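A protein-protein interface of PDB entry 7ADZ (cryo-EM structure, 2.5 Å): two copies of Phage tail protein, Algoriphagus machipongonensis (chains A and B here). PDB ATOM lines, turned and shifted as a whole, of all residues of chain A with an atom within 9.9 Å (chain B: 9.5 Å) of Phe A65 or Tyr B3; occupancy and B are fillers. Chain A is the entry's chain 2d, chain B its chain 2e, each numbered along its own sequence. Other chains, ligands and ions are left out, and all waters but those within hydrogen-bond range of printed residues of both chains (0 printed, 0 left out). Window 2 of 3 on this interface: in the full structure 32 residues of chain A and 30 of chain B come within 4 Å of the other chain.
Phe A65 touches just these residues of chain B: Tyr B3, Pro B4 and Asn B141.
Printed residues of chain A within 4 Å of Tyr B3: Phe A65 (3.6 Å).
Of the printed residues of chain B, Thr A64 touches Pro B4 (3.4 Å) and Leu B5 (3.2 Å).
No residue of chain A comes within 4 Å of Ser B2.
Of chain A, only Thr A64, Phe A65 and Val A125 come within 4 Å of Pro B4.
Of the printed residues of chain B, Ala A126 touches Leu B5 (2.9 Å).
Printed residues of chain A within 4 Å of Asn B141: Phe A65, Ser A67, Asp A68 and Asn A69.
Of the printed residues of chain B, Ser A67 touches Asn B141 (3.2 Å) and Glu B142 (3.5 Å).
Printed residues of chain B within 4 Å of Asn A69: Asn B141 (3.5 Å).
Printed residues of chain B within 4 Å of Val A125: Pro B4 and Leu B5.
Tyr A71 touches none of the printed residues of chain B.
Ile A127 touches none of the printed residues of chain B.
No position is printed for both chains.
Printed residues of chain B that touch a printed residue of chain A: Tyr B3, Pro B4, Leu B5, Asn B141 and Glu B142.
Hydrophobic or aromatic side chains of chain B within 4 Å of the printed part of chain A: Pro B4 and Leu B5.
Along chain B the printed residues that touch a printed residue of chain A span positions 3 to 142.
Of the 21 printed residues of chain A, 7 touch a printed residue of chain B.
Hydrophobic or aromatic side chains of chain A that line the printed part of chain B: Phe A65, Val A125 and Ala A126.
Among the printed residues, 12 pairs touch across the chains.
The side-chain carboxylate (OD2) of Asp A68 lies within salt-bridge range of the side-chain amino group (NZ) of Lys A18, at 2.9 Å.
NH2 of Arg A62 is in salt-bridge range of OD1 of Asp A68.
N of Thr A64 lies within hydrogen-bond range of O of Ala A126, at 3.0 Å.
OD1 of Asp A68 sits close to N of Glu A70 (3.2 Å).
OE2 of Glu B142 lies within hydrogen-bond range of NE2 of Gln B140.
Among the printed residues, pairs that only touch across the chains: Thr A64 with Pro B4 (3.4 Å), Asn A69 with Asn B141 (3.5 Å), Ser A67 with Glu B142 (3.5 Å), Phe A65 with Tyr B3 (3.6 Å), Phe A65 with Pro B4 (3.6 Å), Val A125 with Pro B4 (3.8 Å) and Val A125 with Leu B5 (3.9 Å).
O of Thr A64 lies within hydrogen-bond range of N of Leu B5, 3.2 Å away.
The side-chain amide nitrogen (ND2) of Asn B141 lies within hydrogen-bond range of the backbone carbonyl oxygen (O) of Phe A65, at 3.2 Å.
The backbone NH (N) of Ser A67 sits at hydrogen-bond distance from the side-chain amide oxygen (OD1) of Asn B141, at 3.2 Å.
The backbone carbonyl oxygen (O) of Asp A68 sits at hydrogen-bond distance from the side-chain amide nitrogen (ND2) of Asn B141 (3.5 Å).
The backbone NH (N) of Ala A126 sits at hydrogen-bond distance from the backbone carbonyl oxygen (O) of Leu B5 (2.9 Å).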
ATOM      1  N   LYS A  18     -21.537  -0.686  30.123  1.00  0.00           N
ATOM      2  CA  LYS A  18     -22.101  -1.146  28.852  1.00  0.00           C
ATOM      3  C   LYS A  18     -21.139  -0.875  27.709  1.00  0.00           C
ATOM      4  O   LYS A  18     -20.412   0.120  27.732  1.00  0.00           O
ATOM      5  CB  LYS A  18     -23.418  -0.451  28.523  1.00  0.00           C
ATOM      6  CG  LYS A  18     -24.590  -0.724  29.435  1.00  0.00           C
ATOM      7  CD  LYS A  18     -25.806   0.097  28.942  1.00  0.00           C
ATOM      8  CE  LYS A  18     -27.080  -0.123  29.753  1.00  0.00           C
ATOM      9  NZ  LYS A  18     -26.901   0.280  31.168  1.00  0.00           N
ATOM     10  N   ILE A  19     -21.190  -1.717  26.673  1.00  0.00           N
ATOM     11  CA  ILE A  19     -20.335  -1.534  25.500  1.00  0.00           C
ATOM     12  C   ILE A  19     -21.074  -1.210  24.201  1.00  0.00           C
ATOM     13  O   ILE A  19     -20.445  -1.131  23.139  1.00  0.00           O
ATOM     14  CB  ILE A  19     -19.464  -2.787  25.288  1.00  0.00           C
ATOM     15  CG1 ILE A  19     -20.365  -4.026  25.019  1.00  0.00           C
ATOM     16  CG2 ILE A  19     -18.567  -2.984  26.496  1.00  0.00           C
ATOM     17  CD1 ILE A  19     -19.642  -5.253  24.562  1.00  0.00           C
ATOM     18  N   GLY A  20     -22.402  -1.071  24.264  1.00  0.00           N
ATOM     19  CA  GLY A  20     -23.181  -0.763  23.069  1.00  0.00           C
ATOM     20  C   GLY A  20     -23.427   0.730  22.896  1.00  0.00           C
ATOM     21  O   GLY A  20     -23.817   1.421  23.836  1.00  0.00           O
ATOM     22  N   PHE A  21     -23.252   1.191  21.667  1.00  0.00           N
ATOM     23  CA  PHE A  21     -23.437   2.569  21.229  1.00  0.00           C
ATOM     24  C   PHE A  21     -24.173   2.606  19.912  1.00  0.00           C
ATOM     25  O   PHE A  21     -24.186   1.612  19.191  1.00  0.00           O
ATOM     26  CB  PHE A  21     -22.093   3.303  21.134  1.00  0.00           C
ATOM     27  CG  PHE A  21     -21.435   3.533  22.460  1.00  0.00           C
ATOM     28  CD1 PHE A  21     -20.704   2.567  23.090  1.00  0.00           C
ATOM     29  CD2 PHE A  21     -21.551   4.753  23.076  1.00  0.00           C
ATOM     30  CE1 PHE A  21     -20.131   2.806  24.308  1.00  0.00           C
ATOM     31  CE2 PHE A  21     -20.968   4.987  24.283  1.00  0.00           C
ATOM     32  CZ  PHE A  21     -20.264   4.011  24.898  1.00  0.00           C
ATOM     33  N   THR A  22     -24.787   3.737  19.594  1.00  0.00           N
ATOM     34  CA  THR A  22     -25.478   3.860  18.319  1.00  0.00           C
ATOM     35  C   THR A  22     -24.620   4.571  17.289  1.00  0.00           C
ATOM     36  O   THR A  22     -24.808   4.390  16.088  1.00  0.00           O
ATOM     37  CB  THR A  22     -26.798   4.634  18.476  1.00  0.00           C
ATOM     38  OG1 THR A  22     -26.521   5.954  18.928  1.00  0.00           O
ATOM     39  CG2 THR A  22     -27.675   3.956  19.483  1.00  0.00           C
ATOM     40  N   LYS A  61     -22.303   8.297  20.928  1.00  0.00           N
ATOM     41  CA  LYS A  61     -23.734   8.482  21.221  1.00  0.00           C
ATOM     42  C   LYS A  61     -24.425   7.180  21.580  1.00  0.00           C
ATOM     43  O   LYS A  61     -24.090   6.119  21.037  1.00  0.00           O
ATOM     44  CB  LYS A  61     -24.477   9.028  20.028  1.00  0.00           C
ATOM     45  CG  LYS A  61     -23.986  10.304  19.526  1.00  0.00           C
ATOM     46  CD  LYS A  61     -24.877  10.808  18.463  1.00  0.00           C
ATOM     47  CE  LYS A  61     -24.346  12.052  17.834  1.00  0.00           C
ATOM     48  NZ  LYS A  61     -25.215  12.493  16.728  1.00  0.00           N
ATOM     49  N   ARG A  62     -25.445   7.280  22.436  1.00  0.00           N
ATOM     50  CA  ARG A  62     -26.268   6.130  22.821  1.00  0.00           C
ATOM     51  C   ARG A  62     -27.612   6.590  23.390  1.00  0.00           C
ATOM     52  O   ARG A  62     -27.781   7.779  23.650  1.00  0.00           O
ATOM     53  CB  ARG A  62     -25.559   5.271  23.852  1.00  0.00           C
ATOM     54  CG  ARG A  62     -25.389   5.926  25.182  1.00  0.00           C
ATOM     55  CD  ARG A  62     -24.716   5.079  26.152  1.00  0.00           C
ATOM     56  NE  ARG A  62     -24.775   5.706  27.443  1.00  0.00           N
ATOM     57  CZ  ARG A  62     -24.582   5.115  28.635  1.00  0.00           C
ATOM     58  NH1 ARG A  62     -24.253   3.845  28.752  1.00  0.00           N
ATOM     59  NH2 ARG A  62     -24.784   5.848  29.701  1.00  0.00           N
ATOM     60  N   GLY A  63     -28.556   5.666  23.594  1.00  0.00           N
ATOM     61  CA  GLY A  63     -29.834   6.027  24.214  1.00  0.00           C
ATOM     62  C   GLY A  63     -29.729   6.102  25.724  1.00  0.00           C
ATOM     63  O   GLY A  63     -28.793   5.554  26.306  1.00  0.00           O
ATOM     64  N   THR A  64     -30.722   6.714  26.367  1.00  0.00           N
ATOM     65  CA  THR A  64     -30.704   6.798  27.821  1.00  0.00           C
ATOM     66  C   THR A  64     -31.514   5.684  28.443  1.00  0.00           C
ATOM     67  O   THR A  64     -32.544   5.275  27.914  1.00  0.00           O
ATOM     68  CB  THR A  64     -31.312   8.111  28.312  1.00  0.00           C
ATOM     69  OG1 THR A  64     -32.686   8.129  27.966  1.00  0.00           O
ATOM     70  CG2 THR A  64     -30.633   9.282  27.640  1.00  0.00           C
ATOM     71  N   PHE A  65     -31.092   5.259  29.622  1.00  0.00           N
ATOM     72  CA  PHE A  65     -31.750   4.204  30.375  1.00  0.00           C
ATOM     73  C   PHE A  65     -31.973   4.547  31.826  1.00  0.00           C
ATOM     74  O   PHE A  65     -31.225   5.321  32.427  1.00  0.00           O
ATOM     75  CB  PHE A  65     -30.945   2.912  30.287  1.00  0.00           C
ATOM     76  CG  PHE A  65     -30.896   2.315  28.925  1.00  0.00           C
ATOM     77  CD1 PHE A  65     -30.014   2.760  27.966  1.00  0.00           C
ATOM     78  CD2 PHE A  65     -31.732   1.276  28.603  1.00  0.00           C
ATOM     79  CE1 PHE A  65     -29.991   2.207  26.728  1.00  0.00           C
ATOM     80  CE2 PHE A  65     -31.698   0.713  27.361  1.00  0.00           C
ATOM     81  CZ  PHE A  65     -30.831   1.186  26.421  1.00  0.00           C
ATOM     82  N   LYS A  66     -32.998   3.944  32.394  1.00  0.00           N
ATOM     83  CA  LYS A  66     -33.271   4.085  33.805  1.00  0.00           C
ATOM     84  C   LYS A  66     -32.069   3.627  34.617  1.00  0.00           C
ATOM     85  O   LYS A  66     -31.518   2.558  34.364  1.00  0.00           O
ATOM     86  CB  LYS A  66     -34.507   3.274  34.175  1.00  0.00           C
ATOM     87  CG  LYS A  66     -34.940   3.400  35.607  1.00  0.00           C
ATOM     88  CD  LYS A  66     -36.207   2.614  35.868  1.00  0.00           C
ATOM     89  CE  LYS A  66     -36.625   2.727  37.323  1.00  0.00           C
ATOM     90  NZ  LYS A  66     -37.858   1.947  37.610  1.00  0.00           N
ATOM     91  N   SER A  67     -31.671   4.461  35.571  1.00  0.00           N
ATOM     92  CA  SER A  67     -30.565   4.253  36.509  1.00  0.00           C
ATOM     93  C   SER A  67     -29.144   4.215  35.930  1.00  0.00           C
ATOM     94  O   SER A  67     -28.200   3.906  36.656  1.00  0.00           O
ATOM     95  CB  SER A  67     -30.800   2.991  37.316  1.00  0.00           C
ATOM     96  OG  SER A  67     -32.002   3.065  38.032  1.00  0.00           O
ATOM     97  N   ASP A  68     -28.950   4.564  34.662  1.00  0.00           N
ATOM     98  CA  ASP A  68     -27.594   4.613  34.121  1.00  0.00           C
ATOM     99  C   ASP A  68     -27.094   6.045  34.006  1.00  0.00           C
ATOM    100  O   ASP A  68     -27.515   6.792  33.126  1.00  0.00           O
ATOM    101  CB  ASP A  68     -27.505   3.898  32.782  1.00  0.00           C
ATOM    102  CG  ASP A  68     -26.045   3.870  32.159  1.00  0.00           C
ATOM    103  OD1 ASP A  68     -25.209   4.733  32.465  1.00  0.00           O
ATOM    104  OD2 ASP A  68     -25.788   2.955  31.375  1.00  0.00           O
ATOM    105  N   ASN A  69     -26.369   6.517  35.011  1.00  0.00           N
ATOM    106  CA  ASN A  69     -25.902   7.909  35.089  1.00  0.00           C
ATOM    107  C   ASN A  69     -24.405   8.060  34.850  1.00  0.00           C
ATOM    108  O   ASN A  69     -23.796   8.992  35.323  1.00  0.00           O
ATOM    109  CB  ASN A  69     -26.309   8.560  36.431  1.00  0.00           C
ATOM    110  CG  ASN A  69     -26.523  10.078  36.334  1.00  0.00           C
ATOM    111  OD1 ASN A  69     -27.106  10.569  35.400  1.00  0.00           O
ATOM    112  ND2 ASN A  69     -26.066  10.806  37.318  1.00  0.00           N
ATOM    113  N   GLU A  70     -23.828   7.137  34.093  1.00  0.00           N
ATOM    114  CA  GLU A  70     -22.391   7.075  33.821  1.00  0.00           C
ATOM    115  C   GLU A  70     -21.735   8.228  33.114  1.00  0.00           C
ATOM    116  O   GLU A  70     -20.648   8.582  33.462  1.00  0.00           O
ATOM    117  CB  GLU A  70     -22.063   5.865  32.983  1.00  0.00           C
ATOM    118  CG  GLU A  70     -22.645   4.579  33.476  1.00  0.00           C
ATOM    119  CD  GLU A  70     -21.783   3.981  34.529  1.00  0.00           C
ATOM    120  OE1 GLU A  70     -21.166   4.766  35.245  1.00  0.00           O
ATOM    121  OE2 GLU A  70     -21.717   2.752  34.623  1.00  0.00           O
ATOM    122  N   TYR A  71     -22.363   8.804  32.108  1.00  0.00           N
ATOM    123  CA  TYR A  71     -21.724   9.917  31.410  1.00  0.00           C
ATOM    124  C   TYR A  71     -21.468  11.055  32.402  1.00  0.00           C
ATOM    125  O   TYR A  71     -20.390  11.620  32.421  1.00  0.00           O
ATOM    126  CB  TYR A  71     -22.608  10.459  30.281  1.00  0.00           C
ATOM    127  CG  TYR A  71     -22.541   9.789  28.927  1.00  0.00           C
ATOM    128  CD1 TYR A  71     -23.016  10.445  27.800  1.00  0.00           C
ATOM    129  CD2 TYR A  71     -22.006   8.531  28.763  1.00  0.00           C
ATOM    130  CE1 TYR A  71     -22.988   9.862  26.562  1.00  0.00           C
ATOM    131  CE2 TYR A  71     -21.969   7.940  27.519  1.00  0.00           C
ATOM    132  CZ  TYR A  71     -22.451   8.622  26.422  1.00  0.00           C
ATOM    133  OH  TYR A  71     -22.420   8.064  25.179  1.00  0.00           O
ATOM    134  N   THR A 116     -30.380  15.155  26.142  1.00  0.00           N
ATOM    135  CA  THR A 116     -31.544  15.030  25.276  1.00  0.00           C
ATOM    136  C   THR A 116     -32.477  16.243  25.230  1.00  0.00           C
ATOM    137  O   THR A 116     -32.809  16.811  26.267  1.00  0.00           O
ATOM    138  CB  THR A 116     -32.363  13.836  25.759  1.00  0.00           C
ATOM    139  OG1 THR A 116     -31.544  12.684  25.743  1.00  0.00           O
ATOM    140  CG2 THR A 116     -33.553  13.601  24.922  1.00  0.00           C
ATOM    141  N   VAL A 125     -36.620   8.157  20.545  1.00  0.00           N
ATOM    142  CA  VAL A 125     -35.770   7.730  21.640  1.00  0.00           C
ATOM    143  C   VAL A 125     -34.932   8.862  22.186  1.00  0.00           C
ATOM    144  O   VAL A 125     -34.386   9.655  21.430  1.00  0.00           O
ATOM    145  CB  VAL A 125     -34.848   6.591  21.169  1.00  0.00           C
ATOM    146  CG1 VAL A 125     -33.849   6.193  22.252  1.00  0.00           C
ATOM    147  CG2 VAL A 125     -35.689   5.420  20.800  1.00  0.00           C
ATOM    148  N   ALA A 126     -34.843   8.949  23.503  1.00  0.00           N
ATOM    149  CA  ALA A 126     -33.980   9.930  24.128  1.00  0.00           C
ATOM    150  C   ALA A 126     -32.524   9.523  23.930  1.00  0.00           C
ATOM    151  O   ALA A 126     -32.120   8.438  24.358  1.00  0.00           O
ATOM    152  CB  ALA A 126     -34.289  10.019  25.604  1.00  0.00           C
ATOM    153  N   ILE A 127     -31.750  10.388  23.287  1.00  0.00           N
ATOM    154  CA  ILE A 127     -30.343  10.161  22.968  1.00  0.00           C
ATOM    155  C   ILE A 127     -29.461  11.138  23.700  1.00  0.00           C
ATOM    156  O   ILE A 127     -29.792  12.321  23.779  1.00  0.00           O
ATOM    157  CB  ILE A 127     -30.069  10.276  21.436  1.00  0.00           C
ATOM    158  CG1 ILE A 127     -30.936   9.272  20.623  1.00  0.00           C
ATOM    159  CG2 ILE A 127     -28.569  10.097  21.098  1.00  0.00           C
ATOM    160  CD1 ILE A 127     -30.715   7.800  20.901  1.00  0.00           C
ATOM    161  N   GLU A 128     -28.357  10.634  24.240  1.00  0.00           N
ATOM    162  CA  GLU A 128     -27.363  11.445  24.938  1.00  0.00           C
ATOM    163  C   GLU A 128     -26.010  11.304  24.242  1.00  0.00           C
ATOM    164  O   GLU A 128     -25.729  10.277  23.613  1.00  0.00           O
ATOM    165  CB  GLU A 128     -27.243  11.020  26.402  1.00  0.00           C
ATOM    166  CG  GLU A 128     -26.801   9.573  26.625  1.00  0.00           C
ATOM    167  CD  GLU A 128     -26.650   9.234  28.058  1.00  0.00           C
ATOM    168  OE1 GLU A 128     -27.129   9.986  28.868  1.00  0.00           O
ATOM    169  OE2 GLU A 128     -26.035   8.232  28.366  1.00  0.00           O
ATOM    170  N   SER B   2     -34.190  -4.865  27.913  1.00  0.00           N
ATOM    171  CA  SER B   2     -34.267  -3.475  28.329  1.00  0.00           C
ATOM    172  C   SER B   2     -34.519  -2.552  27.164  1.00  0.00           C
ATOM    173  O   SER B   2     -34.009  -2.762  26.064  1.00  0.00           O
ATOM    174  CB  SER B   2     -32.985  -3.073  29.020  1.00  0.00           C
ATOM    175  OG  SER B   2     -32.808  -3.793  30.206  1.00  0.00           O
ATOM    176  N   TYR B   3     -35.309  -1.519  27.416  1.00  0.00           N
ATOM    177  CA  TYR B   3     -35.648  -0.551  26.403  1.00  0.00           C
ATOM    178  C   TYR B   3     -35.269   0.844  26.888  1.00  0.00           C
ATOM    179  O   TYR B   3     -35.274   1.079  28.092  1.00  0.00           O
ATOM    180  CB  TYR B   3     -37.141  -0.653  26.103  1.00  0.00           C
ATOM    181  CG  TYR B   3     -37.521  -1.982  25.520  1.00  0.00           C
ATOM    182  CD1 TYR B   3     -37.848  -3.032  26.341  1.00  0.00           C
ATOM    183  CD2 TYR B   3     -37.531  -2.153  24.162  1.00  0.00           C
ATOM    184  CE1 TYR B   3     -38.173  -4.246  25.807  1.00  0.00           C
ATOM    185  CE2 TYR B   3     -37.860  -3.366  23.629  1.00  0.00           C
ATOM    186  CZ  TYR B   3     -38.176  -4.409  24.446  1.00  0.00           C
ATOM    187  OH  TYR B   3     -38.496  -5.623  23.906  1.00  0.00           O
ATOM    188  N   PRO B   4     -34.898   1.764  25.991  1.00  0.00           N
ATOM    189  CA  PRO B   4     -34.580   3.150  26.256  1.00  0.00           C
ATOM    190  C   PRO B   4     -35.823   3.959  26.577  1.00  0.00           C
ATOM    191  O   PRO B   4     -36.930   3.555  26.231  1.00  0.00           O
ATOM    192  CB  PRO B   4     -33.927   3.586  24.950  1.00  0.00           C
ATOM    193  CG  PRO B   4     -34.539   2.705  23.910  1.00  0.00           C
ATOM    194  CD  PRO B   4     -34.747   1.390  24.577  1.00  0.00           C
ATOM    195  N   LEU B   5     -35.631   5.111  27.199  1.00  0.00           N
ATOM    196  CA  LEU B   5     -36.722   6.027  27.494  1.00  0.00           C
ATOM    197  C   LEU B   5     -37.071   6.888  26.280  1.00  0.00           C
ATOM    198  O   LEU B   5     -36.191   7.254  25.502  1.00  0.00           O
ATOM    199  CB  LEU B   5     -36.284   6.963  28.630  1.00  0.00           C
ATOM    200  CG  LEU B   5     -35.910   6.320  29.998  1.00  0.00           C
ATOM    201  CD1 LEU B   5     -35.346   7.383  30.903  1.00  0.00           C
ATOM    202  CD2 LEU B   5     -37.118   5.713  30.644  1.00  0.00           C
ATOM    203  N   SER B   6     -38.348   7.242  26.146  1.00  0.00           N
ATOM    204  CA  SER B   6     -38.832   8.163  25.118  1.00  0.00           C
ATOM    205  C   SER B   6     -38.688   9.597  25.608  1.00  0.00           C
ATOM    206  O   SER B   6     -38.386   9.819  26.778  1.00  0.00           O
ATOM    207  CB  SER B   6     -40.261   7.840  24.751  1.00  0.00           C
ATOM    208  OG  SER B   6     -41.123   8.104  25.807  1.00  0.00           O
ATOM    209  N   LEU B  92     -38.097  14.298  33.516  1.00  0.00           N
ATOM    210  CA  LEU B  92     -38.566  13.290  32.550  1.00  0.00           C
ATOM    211  C   LEU B  92     -39.347  12.231  33.334  1.00  0.00           C
ATOM    212  O   LEU B  92     -38.820  11.678  34.309  1.00  0.00           O
ATOM    213  CB  LEU B  92     -37.364  12.688  31.816  1.00  0.00           C
ATOM    214  CG  LEU B  92     -37.606  11.659  30.711  1.00  0.00           C
ATOM    215  CD1 LEU B  92     -38.322  12.314  29.524  1.00  0.00           C
ATOM    216  CD2 LEU B  92     -36.270  11.101  30.279  1.00  0.00           C
ATOM    217  N   VAL B 100     -38.039  10.292  36.673  1.00  0.00           N
ATOM    218  CA  VAL B 100     -37.037   9.277  36.393  1.00  0.00           C
ATOM    219  C   VAL B 100     -35.692   9.989  36.285  1.00  0.00           C
ATOM    220  O   VAL B 100     -34.734   9.614  36.949  1.00  0.00           O
ATOM    221  CB  VAL B 100     -37.334   8.518  35.092  1.00  0.00           C
ATOM    222  CG1 VAL B 100     -36.246   7.482  34.823  1.00  0.00           C
ATOM    223  CG2 VAL B 100     -38.659   7.878  35.185  1.00  0.00           C
ATOM    224  N   VAL B 101     -35.624  11.002  35.415  1.00  0.00           N
ATOM    225  CA  VAL B 101     -34.378  11.754  35.216  1.00  0.00           C
ATOM    226  C   VAL B 101     -34.626  13.224  35.519  1.00  0.00           C
ATOM    227  O   VAL B 101     -35.516  13.848  34.939  1.00  0.00           O
ATOM    228  CB  VAL B 101     -33.831  11.634  33.778  1.00  0.00           C
ATOM    229  CG1 VAL B 101     -32.524  12.431  33.647  1.00  0.00           C
ATOM    230  CG2 VAL B 101     -33.642  10.211  33.433  1.00  0.00           C
ATOM    231  N   GLN B 140     -29.440  14.194  37.854  1.00  0.00           N
ATOM    232  CA  GLN B 140     -29.753  13.076  38.728  1.00  0.00           C
ATOM    233  C   GLN B 140     -30.547  11.955  38.050  1.00  0.00           C
ATOM    234  O   GLN B 140     -31.632  12.160  37.509  1.00  0.00           O
ATOM    235  CB  GLN B 140     -30.543  13.591  39.923  1.00  0.00           C
ATOM    236  CG  GLN B 140     -30.907  12.548  40.932  1.00  0.00           C
ATOM    237  CD  GLN B 140     -31.651  13.133  42.072  1.00  0.00           C
ATOM    238  OE1 GLN B 140     -32.463  14.045  41.897  1.00  0.00           O
ATOM    239  NE2 GLN B 140     -31.391  12.657  43.266  1.00  0.00           N
ATOM    240  N   ASN B 141     -30.018  10.745  38.120  1.00  0.00           N
ATOM    241  CA  ASN B 141     -30.667   9.564  37.546  1.00  0.00           C
ATOM    242  C   ASN B 141     -30.282   8.370  38.392  1.00  0.00           C
ATOM    243  O   ASN B 141     -29.201   7.808  38.230  1.00  0.00           O
ATOM    244  CB  ASN B 141     -30.265   9.361  36.098  1.00  0.00           C
ATOM    245  CG  ASN B 141     -30.988   8.225  35.425  1.00  0.00           C
ATOM    246  OD1 ASN B 141     -31.887   7.612  35.997  1.00  0.00           O
ATOM    247  ND2 ASN B 141     -30.607   7.931  34.212  1.00  0.00           N
ATOM    248  N   GLU B 142     -31.134   8.017  39.337  1.00  0.00           N
ATOM    249  CA  GLU B 142     -30.810   6.996  40.318  1.00  0.00           C
ATOM    250  C   GLU B 142     -31.691   5.769  40.170  1.00  0.00           C
ATOM    251  O   GLU B 142     -32.875   5.802  40.503  1.00  0.00           O
ATOM    252  CB  GLU B 142     -30.966   7.590  41.718  1.00  0.00           C
ATOM    253  CG  GLU B 142     -30.032   8.766  41.990  1.00  0.00           C
ATOM    254  CD  GLU B 142     -30.216   9.397  43.340  1.00  0.00           C
ATOM    255  OE1 GLU B 142     -30.996   8.906  44.113  1.00  0.00           O
ATOM    256  OE2 GLU B 142     -29.602  10.411  43.578  1.00  0.00           O
